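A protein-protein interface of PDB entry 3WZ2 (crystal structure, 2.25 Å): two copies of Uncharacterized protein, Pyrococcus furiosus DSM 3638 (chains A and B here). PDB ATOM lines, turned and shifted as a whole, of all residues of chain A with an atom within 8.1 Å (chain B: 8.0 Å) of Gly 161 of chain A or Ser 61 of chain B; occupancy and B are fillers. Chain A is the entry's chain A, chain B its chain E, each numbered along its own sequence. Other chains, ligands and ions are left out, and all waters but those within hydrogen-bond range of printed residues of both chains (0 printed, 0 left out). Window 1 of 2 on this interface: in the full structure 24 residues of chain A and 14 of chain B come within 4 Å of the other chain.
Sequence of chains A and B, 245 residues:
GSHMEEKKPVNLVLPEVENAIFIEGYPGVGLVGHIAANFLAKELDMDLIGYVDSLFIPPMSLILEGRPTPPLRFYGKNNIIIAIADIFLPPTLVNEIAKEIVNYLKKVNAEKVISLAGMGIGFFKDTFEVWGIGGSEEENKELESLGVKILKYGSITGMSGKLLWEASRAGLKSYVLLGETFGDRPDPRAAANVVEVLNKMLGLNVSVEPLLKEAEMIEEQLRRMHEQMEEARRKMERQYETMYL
The backbone carbonyl oxygen of Gly 154 of chain A is in hydrogen-bond range of the backbone NH of Ile 63 of chain B. O of Ser 61 of chain B sits at hydrogen-bond distance from N of Ile 156 of chain A (2.8 Å). The backbone NH (N) of Gly 158 of chain A lies within hydrogen-bond range of the backbone carbonyl oxygen (O) of Pro 59 of chain B (2.9 Å). The side-chain hydroxyl (OG) of Ser 61 of chain B sits at hydrogen-bond distance from the backbone carbonyl oxygen (O) of Gly 161 of chain A, 2.6 Å away.
The side-chain amide oxygen (OD1) of Asn 95 of chain A sits at hydrogen-bond distance from the side-chain amino group (NZ) of Lys 162 of chain A, 3.1 Å away. N of Val 176 of chain A lies within hydrogen-bond range of O of Ile 133 of chain A (2.9 Å). O of Leu 164 of chain A lies within hydrogen-bond range of OG of Ser 168 of chain A. The backbone carbonyl oxygen of Trp 165 of chain A is in hydrogen-bond range of the side-chain hydroxyl of Ser 168 of chain A, at 3.0 Å. O of Leu 62 of chain B sits at hydrogen-bond distance from N of Thr 69 of chain B, 2.7 Å away. O of Pro 70 of chain B is in hydrogen-bond range of NH1 of Arg 73 of chain B.
Asn 95 of chain A touches Pro 59 of chain B (OD1 to CB, 3.3 Å). CD1 of Ile 133 of chain A touches CG2 of Ile 63 of chain B, 3.9 Å away. Leu 151 of chain A touches Ile 63 of chain B (O to CG2, 3.6 Å). CA of Met 60 of chain B touches O of Ile 156 of chain A, at 3.2 Å. Thr 157 of chain A touches Pro 59 of chain B. Met 60 of chain B touches Gly 161 of chain A. CB of Lys 162 of chain A touches CB of Pro 59 of chain B (3.98 Å). Pro 68 of chain B touches Leu 164 of chain A. Trp 165 of chain A touches Ser 61 of chain B. Trp 165 of chain A touches Pro 70 of chain B.
Printed residues of chain B within 4 Å of Ile 133 of chain A: Ile 63. Of the printed residues of chain B, Gly 158 of chain A touches Pro 59. Gly 161 of chain A touches two residues of chain B. Ser 168 of chain A touches none of the printed residues of chain B. Printed residues of chain A within 4 Å of Met 60 of chain B: Ile 156 and Gly 161. Printed residues of chain A within 4 Å of Ser 61 of chain B: Ser 155, Ile 156, Gly 161 and Trp 165. Of the printed residues of chain A, Leu 62 of chain B touches Gly 154 and Ser 155. Pro 71 of chain B touches none of the printed residues of chain A. The nearest printed residue of chain B that does not touch Trp 165 of chain A is Thr 69 of chain B (4.3 Å).
Of the 27 printed residues of chain A, 13 touch a printed residue of chain B. Hydrophobic or aromatic side chains of chain A that line the printed part of chain B: Val 94, Ile 133, Leu 164 and Trp 165. Hydrophobic or aromatic side chains of chain B within 4 Å of the printed part of chain A: Pro 59, Met 60, Leu 62, Ile 63, Pro 68 and Pro 70. Along chain B the printed residues that touch a printed residue of chain A span positions 59 to 70.
No position is printed for both chains. Of the 19 pairs that touch across the chains among the printed residues, none has its exchanged pair printed and touching as well.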
ATOM      1  N   GLU A  24     -14.464 -26.681   1.619  1.00  0.00           N
ATOM      2  CA  GLU A  24     -15.296 -26.430   2.750  1.00  0.00           C
ATOM      3  C   GLU A  24     -16.691 -27.019   2.504  1.00  0.00           C
ATOM      4  O   GLU A  24     -17.296 -26.730   1.471  1.00  0.00           O
ATOM      5  CB  GLU A  24     -15.382 -24.918   2.966  1.00  0.00           C
ATOM      6  CG  GLU A  24     -16.419 -24.468   3.962  1.00  0.00           C
ATOM      7  CD  GLU A  24     -17.770 -24.154   3.372  1.00  0.00           C
ATOM      8  OE1 GLU A  24     -17.873 -23.413   2.360  1.00  0.00           O
ATOM      9  OE2 GLU A  24     -18.777 -24.694   3.906  1.00  0.00           O
ATOM     10  N   VAL A  94     -19.695 -17.901  12.637  1.00  0.00           N
ATOM     11  CA  VAL A  94     -19.341 -18.269  11.254  1.00  0.00           C
ATOM     12  C   VAL A  94     -18.429 -17.220  10.665  1.00  0.00           C
ATOM     13  O   VAL A  94     -17.422 -17.569  10.061  1.00  0.00           O
ATOM     14  CB  VAL A  94     -20.591 -18.458  10.377  1.00  0.00           C
ATOM     15  CG1 VAL A  94     -20.229 -18.586   8.906  1.00  0.00           C
ATOM     16  CG2 VAL A  94     -21.371 -19.693  10.842  1.00  0.00           C
ATOM     17  N   ASN A  95     -18.768 -15.940  10.824  1.00  0.00           N
ATOM     18  CA  ASN A  95     -17.879 -14.881  10.300  1.00  0.00           C
ATOM     19  C   ASN A  95     -16.508 -14.903  10.932  1.00  0.00           C
ATOM     20  O   ASN A  95     -15.533 -14.727  10.247  1.00  0.00           O
ATOM     21  CB  ASN A  95     -18.479 -13.499  10.508  1.00  0.00           C
ATOM     22  CG  ASN A  95     -19.635 -13.229   9.586  1.00  0.00           C
ATOM     23  OD1 ASN A  95     -19.658 -13.695   8.428  1.00  0.00           O
ATOM     24  ND2 ASN A  95     -20.591 -12.440  10.063  1.00  0.00           N
ATOM     25  N   ALA A  98     -14.669 -17.870   9.410  1.00  0.00           N
ATOM     26  CA  ALA A  98     -14.282 -17.521   8.028  1.00  0.00           C
ATOM     27  C   ALA A  98     -13.055 -16.618   7.962  1.00  0.00           C
ATOM     28  O   ALA A  98     -12.135 -16.827   7.139  1.00  0.00           O
ATOM     29  CB  ALA A  98     -15.424 -16.887   7.278  1.00  0.00           C
ATOM     30  N   SER A 115     -15.914 -24.202  -2.029  1.00  0.00           N
ATOM     31  CA  SER A 115     -17.015 -24.503  -1.157  1.00  0.00           C
ATOM     32  C   SER A 115     -18.024 -25.451  -1.857  1.00  0.00           C
ATOM     33  O   SER A 115     -18.314 -25.309  -3.039  1.00  0.00           O
ATOM     34  CB  SER A 115     -17.681 -23.202  -0.710  1.00  0.00           C
ATOM     35  OG  SER A 115     -16.785 -22.430   0.087  1.00  0.00           O
ATOM     36  N   ALA A 117     -21.879 -26.682  -1.661  1.00  0.00           N
ATOM     37  CA  ALA A 117     -23.138 -26.153  -1.116  1.00  0.00           C
ATOM     38  C   ALA A 117     -24.324 -26.729  -1.862  1.00  0.00           C
ATOM     39  O   ALA A 117     -24.163 -27.446  -2.865  1.00  0.00           O
ATOM     40  CB  ALA A 117     -23.157 -24.634  -1.238  1.00  0.00           C
ATOM     41  N   ILE A 133     -19.971 -21.124  -9.295  1.00  0.00           N
ATOM     42  CA  ILE A 133     -19.665 -19.708  -9.332  1.00  0.00           C
ATOM     43  C   ILE A 133     -18.236 -19.526  -8.849  1.00  0.00           C
ATOM     44  O   ILE A 133     -17.756 -20.235  -7.965  1.00  0.00           O
ATOM     45  CB  ILE A 133     -20.664 -18.904  -8.508  1.00  0.00           C
ATOM     46  CG1 ILE A 133     -20.371 -17.397  -8.526  1.00  0.00           C
ATOM     47  CG2 ILE A 133     -20.663 -19.360  -7.064  1.00  0.00           C
ATOM     48  CD1 ILE A 133     -20.563 -16.746  -9.891  1.00  0.00           C
ATOM     49  N   LEU A 151     -23.876 -19.833 -12.147  1.00  0.00           N
ATOM     50  CA  LEU A 151     -25.011 -19.121 -11.539  1.00  0.00           C
ATOM     51  C   LEU A 151     -24.907 -17.623 -11.809  1.00  0.00           C
ATOM     52  O   LEU A 151     -23.872 -17.020 -11.561  1.00  0.00           O
ATOM     53  CB  LEU A 151     -25.014 -19.360 -10.029  1.00  0.00           C
ATOM     54  CG  LEU A 151     -26.215 -18.831  -9.255  1.00  0.00           C
ATOM     55  CD1 LEU A 151     -27.520 -19.452  -9.748  1.00  0.00           C
ATOM     56  CD2 LEU A 151     -26.012 -19.089  -7.768  1.00  0.00           C
ATOM     57  N   GLY A 154     -28.392 -14.909  -7.711  1.00  0.00           N
ATOM     58  CA  GLY A 154     -28.990 -15.557  -6.576  1.00  0.00           C
ATOM     59  C   GLY A 154     -28.172 -15.217  -5.350  1.00  0.00           C
ATOM     60  O   GLY A 154     -27.344 -14.330  -5.367  1.00  0.00           O
ATOM     61  N   SER A 155     -28.387 -15.934  -4.285  1.00  0.00           N
ATOM     62  CA  SER A 155     -27.616 -15.683  -3.089  1.00  0.00           C
ATOM     63  C   SER A 155     -27.092 -16.967  -2.499  1.00  0.00           C
ATOM     64  O   SER A 155     -27.719 -18.019  -2.624  1.00  0.00           O
ATOM     65  CB  SER A 155     -28.435 -14.942  -2.069  1.00  0.00           C
ATOM     66  OG  SER A 155     -29.523 -15.717  -1.692  1.00  0.00           O
ATOM     67  N   ILE A 156     -25.914 -16.861  -1.893  1.00  0.00           N
ATOM     68  CA  ILE A 156     -25.310 -17.963  -1.187  1.00  0.00           C
ATOM     69  C   ILE A 156     -25.029 -17.544   0.263  1.00  0.00           C
ATOM     70  O   ILE A 156     -24.178 -16.716   0.497  1.00  0.00           O
ATOM     71  CB  ILE A 156     -24.016 -18.391  -1.882  1.00  0.00           C
ATOM     72  CG1 ILE A 156     -24.273 -18.678  -3.356  1.00  0.00           C
ATOM     73  CG2 ILE A 156     -23.469 -19.628  -1.210  1.00  0.00           C
ATOM     74  CD1 ILE A 156     -23.006 -18.984  -4.138  1.00  0.00           C
ATOM     75  N   THR A 157     -25.778 -18.091   1.203  1.00  0.00           N
ATOM     76  CA  THR A 157     -25.682 -17.725   2.607  1.00  0.00           C
ATOM     77  C   THR A 157     -24.736 -18.659   3.335  1.00  0.00           C
ATOM     78  O   THR A 157     -24.443 -19.751   2.875  1.00  0.00           O
ATOM     79  CB  THR A 157     -27.050 -17.811   3.317  1.00  0.00           C
ATOM     80  OG1 THR A 157     -27.591 -19.124   3.134  1.00  0.00           O
ATOM     81  CG2 THR A 157     -28.030 -16.785   2.727  1.00  0.00           C
ATOM     82  N   GLY A 158     -24.244 -18.217   4.482  1.00  0.00           N
ATOM     83  CA  GLY A 158     -23.446 -19.070   5.327  1.00  0.00           C
ATOM     84  C   GLY A 158     -21.988 -19.027   4.919  1.00  0.00           C
ATOM     85  O   GLY A 158     -21.545 -18.142   4.176  1.00  0.00           O
ATOM     86  N   MET A 159     -21.255 -19.993   5.442  1.00  0.00           N
ATOM     87  CA  MET A 159     -19.837 -20.062   5.304  1.00  0.00           C
ATOM     88  C   MET A 159     -19.447 -20.023   3.840  1.00  0.00           C
ATOM     89  O   MET A 159     -18.507 -19.319   3.473  1.00  0.00           O
ATOM     90  CB  MET A 159     -19.325 -21.342   5.967  1.00  0.00           C
ATOM     91  CG  MET A 159     -17.846 -21.567   5.817  1.00  0.00           C
ATOM     92  SD  MET A 159     -16.842 -20.309   6.603  1.00  0.00           S
ATOM     93  CE  MET A 159     -16.906 -20.810   8.340  1.00  0.00           C
ATOM     94  N   SER A 160     -20.177 -20.743   3.003  1.00  0.00           N
ATOM     95  CA  SER A 160     -19.831 -20.844   1.584  1.00  0.00           C
ATOM     96  C   SER A 160     -19.861 -19.472   0.898  1.00  0.00           C
ATOM     97  O   SER A 160     -18.939 -19.137   0.184  1.00  0.00           O
ATOM     98  CB  SER A 160     -20.738 -21.862   0.870  1.00  0.00           C
ATOM     99  OG  SER A 160     -20.441 -23.174   1.373  1.00  0.00           O
ATOM    100  N   GLY A 161     -20.910 -18.699   1.135  1.00  0.00           N
ATOM    101  CA  GLY A 161     -21.008 -17.354   0.622  1.00  0.00           C
ATOM    102  C   GLY A 161     -19.897 -16.430   1.125  1.00  0.00           C
ATOM    103  O   GLY A 161     -19.328 -15.664   0.354  1.00  0.00           O
ATOM    104  N   LYS A 162     -19.583 -16.513   2.413  1.00  0.00           N
ATOM    105  CA  LYS A 162     -18.594 -15.646   3.009  1.00  0.00           C
ATOM    106  C   LYS A 162     -17.225 -15.940   2.494  1.00  0.00           C
ATOM    107  O   LYS A 162     -16.510 -15.034   2.103  1.00  0.00           O
ATOM    108  CB  LYS A 162     -18.597 -15.762   4.554  1.00  0.00           C
ATOM    109  CG  LYS A 162     -17.846 -14.654   5.262  1.00  0.00           C
ATOM    110  CD  LYS A 162     -18.616 -13.336   5.103  1.00  0.00           C
ATOM    111  CE  LYS A 162     -17.788 -12.104   5.413  1.00  0.00           C
ATOM    112  NZ  LYS A 162     -17.549 -11.991   6.865  1.00  0.00           N
ATOM    113  N   LEU A 163     -16.867 -17.217   2.445  1.00  0.00           N
ATOM    114  CA  LEU A 163     -15.602 -17.625   1.920  1.00  0.00           C
ATOM    115  C   LEU A 163     -15.418 -17.244   0.459  1.00  0.00           C
ATOM    116  O   LEU A 163     -14.351 -16.812   0.061  1.00  0.00           O
ATOM    117  CB  LEU A 163     -15.441 -19.150   2.021  1.00  0.00           C
ATOM    118  CG  LEU A 163     -14.787 -19.781   3.254  1.00  0.00           C
ATOM    119  CD1 LEU A 163     -14.370 -21.242   3.081  1.00  0.00           C
ATOM    120  CD2 LEU A 163     -13.646 -18.904   3.748  1.00  0.00           C
ATOM    121  N   LEU A 164     -16.430 -17.466  -0.356  1.00  0.00           N
ATOM    122  CA  LEU A 164     -16.322 -17.143  -1.782  1.00  0.00           C
ATOM    123  C   LEU A 164     -15.825 -15.702  -1.902  1.00  0.00           C
ATOM    124  O   LEU A 164     -14.867 -15.438  -2.598  1.00  0.00           O
ATOM    125  CB  LEU A 164     -17.688 -17.317  -2.447  1.00  0.00           C
ATOM    126  CG  LEU A 164     -17.813 -16.848  -3.888  1.00  0.00           C
ATOM    127  CD1 LEU A 164     -16.908 -17.628  -4.805  1.00  0.00           C
ATOM    128  CD2 LEU A 164     -19.258 -16.923  -4.327  1.00  0.00           C
ATOM    129  N   TRP A 165     -16.463 -14.806  -1.158  1.00  0.00           N
ATOM    130  CA  TRP A 165     -16.198 -13.371  -1.266  1.00  0.00           C
ATOM    131  C   TRP A 165     -14.859 -13.042  -0.638  1.00  0.00           C
ATOM    132  O   TRP A 165     -14.003 -12.435  -1.273  1.00  0.00           O
ATOM    133  CB  TRP A 165     -17.323 -12.563  -0.597  1.00  0.00           C
ATOM    134  CG  TRP A 165     -16.971 -11.113  -0.477  1.00  0.00           C
ATOM    135  CD1 TRP A 165     -16.687 -10.417   0.679  1.00  0.00           C
ATOM    136  CD2 TRP A 165     -16.845 -10.174  -1.559  1.00  0.00           C
ATOM    137  NE1 TRP A 165     -16.402  -9.111   0.362  1.00  0.00           N
ATOM    138  CE2 TRP A 165     -16.486  -8.936  -0.996  1.00  0.00           C
ATOM    139  CE3 TRP A 165     -17.012 -10.264  -2.947  1.00  0.00           C
ATOM    140  CZ2 TRP A 165     -16.279  -7.789  -1.781  1.00  0.00           C
ATOM    141  CZ3 TRP A 165     -16.809  -9.134  -3.733  1.00  0.00           C
ATOM    142  CH2 TRP A 165     -16.443  -7.906  -3.143  1.00  0.00           C
ATOM    143  N   GLU A 166     -14.654 -13.483   0.608  1.00  0.00           N
ATOM    144  CA  GLU A 166     -13.483 -13.031   1.349  1.00  0.00           C
ATOM    145  C   GLU A 166     -12.232 -13.615   0.722  1.00  0.00           C
ATOM    146  O   GLU A 166     -11.208 -12.971   0.691  1.00  0.00           O
ATOM    147  CB  GLU A 166     -13.590 -13.390   2.857  1.00  0.00           C
ATOM    148  CG  GLU A 166     -14.615 -12.545   3.627  1.00  0.00           C
ATOM    149  CD  GLU A 166     -14.288 -11.035   3.628  1.00  0.00           C
ATOM    150  OE1 GLU A 166     -13.074 -10.701   3.666  1.00  0.00           O
ATOM    151  OE2 GLU A 166     -15.219 -10.189   3.613  1.00  0.00           O
ATOM    152  N   ALA A 167     -12.278 -14.870   0.306  1.00  0.00           N
ATOM    153  CA  ALA A 167     -11.107 -15.506  -0.278  1.00  0.00           C
ATOM    154  C   ALA A 167     -10.747 -14.834  -1.607  1.00  0.00           C
ATOM    155  O   ALA A 167      -9.593 -14.580  -1.859  1.00  0.00           O
ATOM    156  CB  ALA A 167     -11.353 -16.996  -0.489  1.00  0.00           C
ATOM    157  N   SER A 168     -11.753 -14.499  -2.415  1.00  0.00           N
ATOM    158  CA  SER A 168     -11.518 -13.802  -3.707  1.00  0.00           C
ATOM    159  C   SER A 168     -10.935 -12.379  -3.450  1.00  0.00           C
ATOM    160  O   SER A 168      -9.921 -12.035  -4.038  1.00  0.00           O
ATOM    161  CB  SER A 168     -12.745 -13.810  -4.647  1.00  0.00           C
ATOM    162  OG  SER A 168     -13.777 -12.998  -4.167  1.00  0.00           O
ATOM    163  N   SER A 174     -11.227 -18.819  -5.849  1.00  0.00           N
ATOM    164  CA  SER A 174     -12.343 -19.164  -5.025  1.00  0.00           C
ATOM    165  C   SER A 174     -13.460 -19.716  -5.904  1.00  0.00           C
ATOM    166  O   SER A 174     -13.694 -19.186  -7.024  1.00  0.00           O
ATOM    167  CB  SER A 174     -12.812 -17.790  -4.454  1.00  0.00           C
ATOM    168  OG  SER A 174     -13.572 -17.877  -3.311  1.00  0.00           O
ATOM    169  N   TYR A 175     -14.153 -20.758  -5.424  1.00  0.00           N
ATOM    170  CA  TYR A 175     -15.272 -21.366  -6.140  1.00  0.00           C
ATOM    171  C   TYR A 175     -16.336 -21.849  -5.163  1.00  0.00           C
ATOM    172  O   TYR A 175     -16.018 -22.257  -4.065  1.00  0.00           O
ATOM    173  CB  TYR A 175     -14.837 -22.582  -6.989  1.00  0.00           C
ATOM    174  CG  TYR A 175     -13.532 -22.491  -7.718  1.00  0.00           C
ATOM    175  CD1 TYR A 175     -13.453 -22.477  -9.126  1.00  0.00           C
ATOM    176  CD2 TYR A 175     -12.367 -22.420  -7.010  1.00  0.00           C
ATOM    177  CE1 TYR A 175     -12.228 -22.431  -9.785  1.00  0.00           C
ATOM    178  CE2 TYR A 175     -11.139 -22.347  -7.647  1.00  0.00           C
ATOM    179  CZ  TYR A 175     -11.072 -22.384  -9.031  1.00  0.00           C
ATOM    180  OH  TYR A 175      -9.853 -22.295  -9.642  1.00  0.00           O
ATOM    181  N   VAL A 176     -17.585 -21.851  -5.603  1.00  0.00           N
ATOM    182  CA  VAL A 176     -18.621 -22.648  -4.976  1.00  0.00           C
ATOM    183  C   VAL A 176     -19.262 -23.584  -6.020  1.00  0.00           C
ATOM    184  O   VAL A 176     -19.615 -23.162  -7.121  1.00  0.00           O
ATOM    185  CB  VAL A 176     -19.703 -21.758  -4.337  1.00  0.00           C
ATOM    186  CG1 VAL A 176     -20.673 -22.581  -3.533  1.00  0.00           C
ATOM    187  CG2 VAL A 176     -19.083 -20.682  -3.475  1.00  0.00           C
ATOM    188  N   LEU A 178     -22.654 -25.792  -6.423  1.00  0.00           N
ATOM    189  CA  LEU A 178     -23.979 -25.855  -5.841  1.00  0.00           C
ATOM    190  C   LEU A 178     -24.808 -26.985  -6.453  1.00  0.00           C
ATOM    191  O   LEU A 178     -25.198 -26.936  -7.621  1.00  0.00           O
ATOM    192  CB  LEU A 178     -24.708 -24.550  -6.051  1.00  0.00           C
ATOM    193  CG  LEU A 178     -24.017 -23.342  -5.398  1.00  0.00           C
ATOM    194  CD1 LEU A 178     -23.440 -22.450  -6.452  1.00  0.00           C
ATOM    195  CD2 LEU A 178     -25.006 -22.554  -4.589  1.00  0.00           C
ATOM    196  N   PRO B  58     -24.551 -10.631   8.580  1.00  0.00           N
ATOM    197  CA  PRO B  58     -24.543 -12.090   8.533  1.00  0.00           C
ATOM    198  C   PRO B  58     -23.875 -12.606   7.252  1.00  0.00           C
ATOM    199  O   PRO B  58     -23.823 -11.889   6.272  1.00  0.00           O
ATOM    200  CB  PRO B  58     -26.028 -12.485   8.597  1.00  0.00           C
ATOM    201  CG  PRO B  58     -26.811 -11.223   8.534  1.00  0.00           C
ATOM    202  CD  PRO B  58     -25.892 -10.062   8.757  1.00  0.00           C
ATOM    203  N   PRO B  59     -23.313 -13.810   7.306  1.00  0.00           N
ATOM    204  CA  PRO B  59     -22.425 -14.321   6.243  1.00  0.00           C
ATOM    205  C   PRO B  59     -23.217 -14.641   5.002  1.00  0.00           C
ATOM    206  O   PRO B  59     -24.205 -15.369   5.087  1.00  0.00           O
ATOM    207  CB  PRO B  59     -21.845 -15.600   6.842  1.00  0.00           C
ATOM    208  CG  PRO B  59     -22.782 -15.982   7.956  1.00  0.00           C
ATOM    209  CD  PRO B  59     -23.383 -14.720   8.464  1.00  0.00           C
ATOM    210  N   MET B  60     -22.797 -14.093   3.871  1.00  0.00           N
ATOM    211  CA  MET B  60     -23.459 -14.327   2.576  1.00  0.00           C
ATOM    212  C   MET B  60     -22.683 -13.646   1.472  1.00  0.00           C
ATOM    213  O   MET B  60     -21.970 -12.689   1.734  1.00  0.00           O
ATOM    214  CB  MET B  60     -24.883 -13.803   2.547  1.00  0.00           C
ATOM    215  CG  MET B  60     -24.966 -12.312   2.579  1.00  0.00           C
ATOM    216  SD  MET B  60     -26.676 -11.785   2.793  1.00  0.00           S
ATOM    217  CE  MET B  60     -27.522 -12.766   1.572  1.00  0.00           C
ATOM    218  N   SER B  61     -22.829 -14.158   0.249  1.00  0.00           N
ATOM    219  CA  SER B  61     -22.617 -13.386  -0.954  1.00  0.00           C
ATOM    220  C   SER B  61     -23.878 -13.363  -1.770  1.00  0.00           C
ATOM    221  O   SER B  61     -24.565 -14.377  -1.884  1.00  0.00           O
ATOM    222  CB  SER B  61     -21.514 -14.011  -1.807  1.00  0.00           C
ATOM    223  OG  SER B  61     -20.279 -13.805  -1.221  1.00  0.00           O
ATOM    224  N   LEU B  62     -24.136 -12.223  -2.381  1.00  0.00           N
ATOM    225  CA  LEU B  62     -25.124 -12.121  -3.409  1.00  0.00           C
ATOM    226  C   LEU B  62     -24.447 -12.267  -4.751  1.00  0.00           C
ATOM    227  O   LEU B  62     -23.369 -11.729  -4.954  1.00  0.00           O
ATOM    228  CB  LEU B  62     -25.805 -10.766  -3.303  1.00  0.00           C
ATOM    229  CG  LEU B  62     -26.521 -10.576  -1.960  1.00  0.00           C
ATOM    230  CD1 LEU B  62     -27.088  -9.188  -1.896  1.00  0.00           C
ATOM    231  CD2 LEU B  62     -27.618 -11.597  -1.709  1.00  0.00           C
ATOM    232  N   ILE B  63     -25.051 -13.037  -5.643  1.00  0.00           N
ATOM    233  CA  ILE B  63     -24.502 -13.205  -6.991  1.00  0.00           C
ATOM    234  C   ILE B  63     -25.308 -12.343  -7.948  1.00  0.00           C
ATOM    235  O   ILE B  63     -26.508 -12.489  -8.041  1.00  0.00           O
ATOM    236  CB  ILE B  63     -24.566 -14.646  -7.503  1.00  0.00           C
ATOM    237  CG1 ILE B  63     -24.043 -15.646  -6.469  1.00  0.00           C
ATOM    238  CG2 ILE B  63     -23.774 -14.754  -8.800  1.00  0.00           C
ATOM    239  CD1 ILE B  63     -22.641 -15.361  -5.975  1.00  0.00           C
ATOM    240  N   LEU B  64     -24.619 -11.418  -8.600  1.00  0.00           N
ATOM    241  CA  LEU B  64     -25.218 -10.463  -9.509  1.00  0.00           C
ATOM    242  C   LEU B  64     -24.389 -10.492 -10.789  1.00  0.00           C
ATOM    243  O   LEU B  64     -23.183 -10.223 -10.741  1.00  0.00           O
ATOM    244  CB  LEU B  64     -25.178  -9.055  -8.900  1.00  0.00           C
ATOM    245  CG  LEU B  64     -26.050  -8.760  -7.646  1.00  0.00           C
ATOM    246  CD1 LEU B  64     -25.917  -7.319  -7.143  1.00  0.00           C
ATOM    247  CD2 LEU B  64     -27.508  -9.063  -7.920  1.00  0.00           C
ATOM    248  N   ARG B  67     -21.157 -12.474 -10.568  1.00  0.00           N
ATOM    249  CA  ARG B  67     -20.085 -11.978  -9.695  1.00  0.00           C
ATOM    250  C   ARG B  67     -20.557 -12.016  -8.246  1.00  0.00           C
ATOM    251  O   ARG B  67     -21.660 -11.562  -7.935  1.00  0.00           O
ATOM    252  CB  ARG B  67     -19.717 -10.553 -10.067  1.00  0.00           C
ATOM    253  CG  ARG B  67     -19.001 -10.474 -11.392  1.00  0.00           C
ATOM    254  CD  ARG B  67     -18.298  -9.145 -11.617  1.00  0.00           C
ATOM    255  NE  ARG B  67     -18.130  -8.858 -13.047  1.00  0.00           N
ATOM    256  CZ  ARG B  67     -17.478  -9.619 -13.945  1.00  0.00           C
ATOM    257  NH1 ARG B  67     -16.891 -10.777 -13.619  1.00  0.00           N
ATOM    258  NH2 ARG B  67     -17.416  -9.212 -15.212  1.00  0.00           N
ATOM    259  N   PRO B  68     -19.725 -12.547  -7.348  1.00  0.00           N
ATOM    260  CA  PRO B  68     -20.101 -12.441  -5.956  1.00  0.00           C
ATOM    261  C   PRO B  68     -19.998 -11.018  -5.423  1.00  0.00           C
ATOM    262  O   PRO B  68     -19.095 -10.282  -5.778  1.00  0.00           O
ATOM    263  CB  PRO B  68     -19.093 -13.321  -5.245  1.00  0.00           C
ATOM    264  CG  PRO B  68     -17.982 -13.496  -6.178  1.00  0.00           C
ATOM    265  CD  PRO B  68     -18.524 -13.356  -7.551  1.00  0.00           C
ATOM    266  N   THR B  69     -20.948 -10.663  -4.586  1.00  0.00           N
ATOM    267  CA  THR B  69     -21.111  -9.330  -4.068  1.00  0.00           C
ATOM    268  C   THR B  69     -21.504  -9.379  -2.601  1.00  0.00           C
ATOM    269  O   THR B  69     -22.345 -10.177  -2.236  1.00  0.00           O
ATOM    270  CB  THR B  69     -22.293  -8.726  -4.876  1.00  0.00           C
ATOM    271  OG1 THR B  69     -21.811  -8.264  -6.143  1.00  0.00           O
ATOM    272  CG2 THR B  69     -22.935  -7.625  -4.207  1.00  0.00           C
ATOM    273  N   PRO B  70     -20.991  -8.450  -1.773  1.00  0.00           N
ATOM    274  CA  PRO B  70     -21.471  -8.394  -0.385  1.00  0.00           C
ATOM    275  C   PRO B  70     -22.791  -7.655  -0.264  1.00  0.00           C
ATOM    276  O   PRO B  70     -23.190  -6.927  -1.163  1.00  0.00           O
ATOM    277  CB  PRO B  70     -20.357  -7.667   0.343  1.00  0.00           C
ATOM    278  CG  PRO B  70     -19.812  -6.742  -0.685  1.00  0.00           C
ATOM    279  CD  PRO B  70     -20.036  -7.373  -2.044  1.00  0.00           C
ATOM    280  N   PRO B  71     -23.513  -7.896   0.827  1.00  0.00           N
ATOM    281  CA  PRO B  71     -24.852  -7.358   0.961  1.00  0.00           C
ATOM    282  C   PRO B  71     -24.939  -5.870   1.229  1.00  0.00           C
ATOM    283  O   PRO B  71     -25.982  -5.293   0.968  1.00  0.00           O
ATOM    284  CB  PRO B  71     -25.423  -8.123   2.155  1.00  0.00           C
ATOM    285  CG  PRO B  71     -24.256  -8.591   2.914  1.00  0.00           C
ATOM    286  CD  PRO B  71     -23.149  -8.794   1.933  1.00  0.00           C
ATOM    287  N   ARG B  73     -23.167  -2.568  -0.017  1.00  0.00           N
ATOM    288  CA  ARG B  73     -22.205  -2.222  -1.045  1.00  0.00           C
ATOM    289  C   ARG B  73     -22.367  -0.777  -1.496  1.00  0.00           C
ATOM    290  O   ARG B  73     -23.402  -0.136  -1.267  1.00  0.00           O
ATOM    291  CB  ARG B  73     -22.221  -3.196  -2.241  1.00  0.00           C
ATOM    292  CG  ARG B  73     -23.571  -3.613  -2.692  1.00  0.00           C
ATOM    293  CD  ARG B  73     -23.557  -4.748  -3.713  1.00  0.00           C
ATOM    294  NE  ARG B  73     -24.899  -4.785  -4.262  1.00  0.00           N
ATOM    295  CZ  ARG B  73     -25.941  -5.311  -3.641  1.00  0.00           C
ATOM    296  NH1 ARG B  73     -25.800  -5.894  -2.454  1.00  0.00           N
ATOM    297  NH2 ARG B  73     -27.123  -5.264  -4.198  1.00  0.00           N
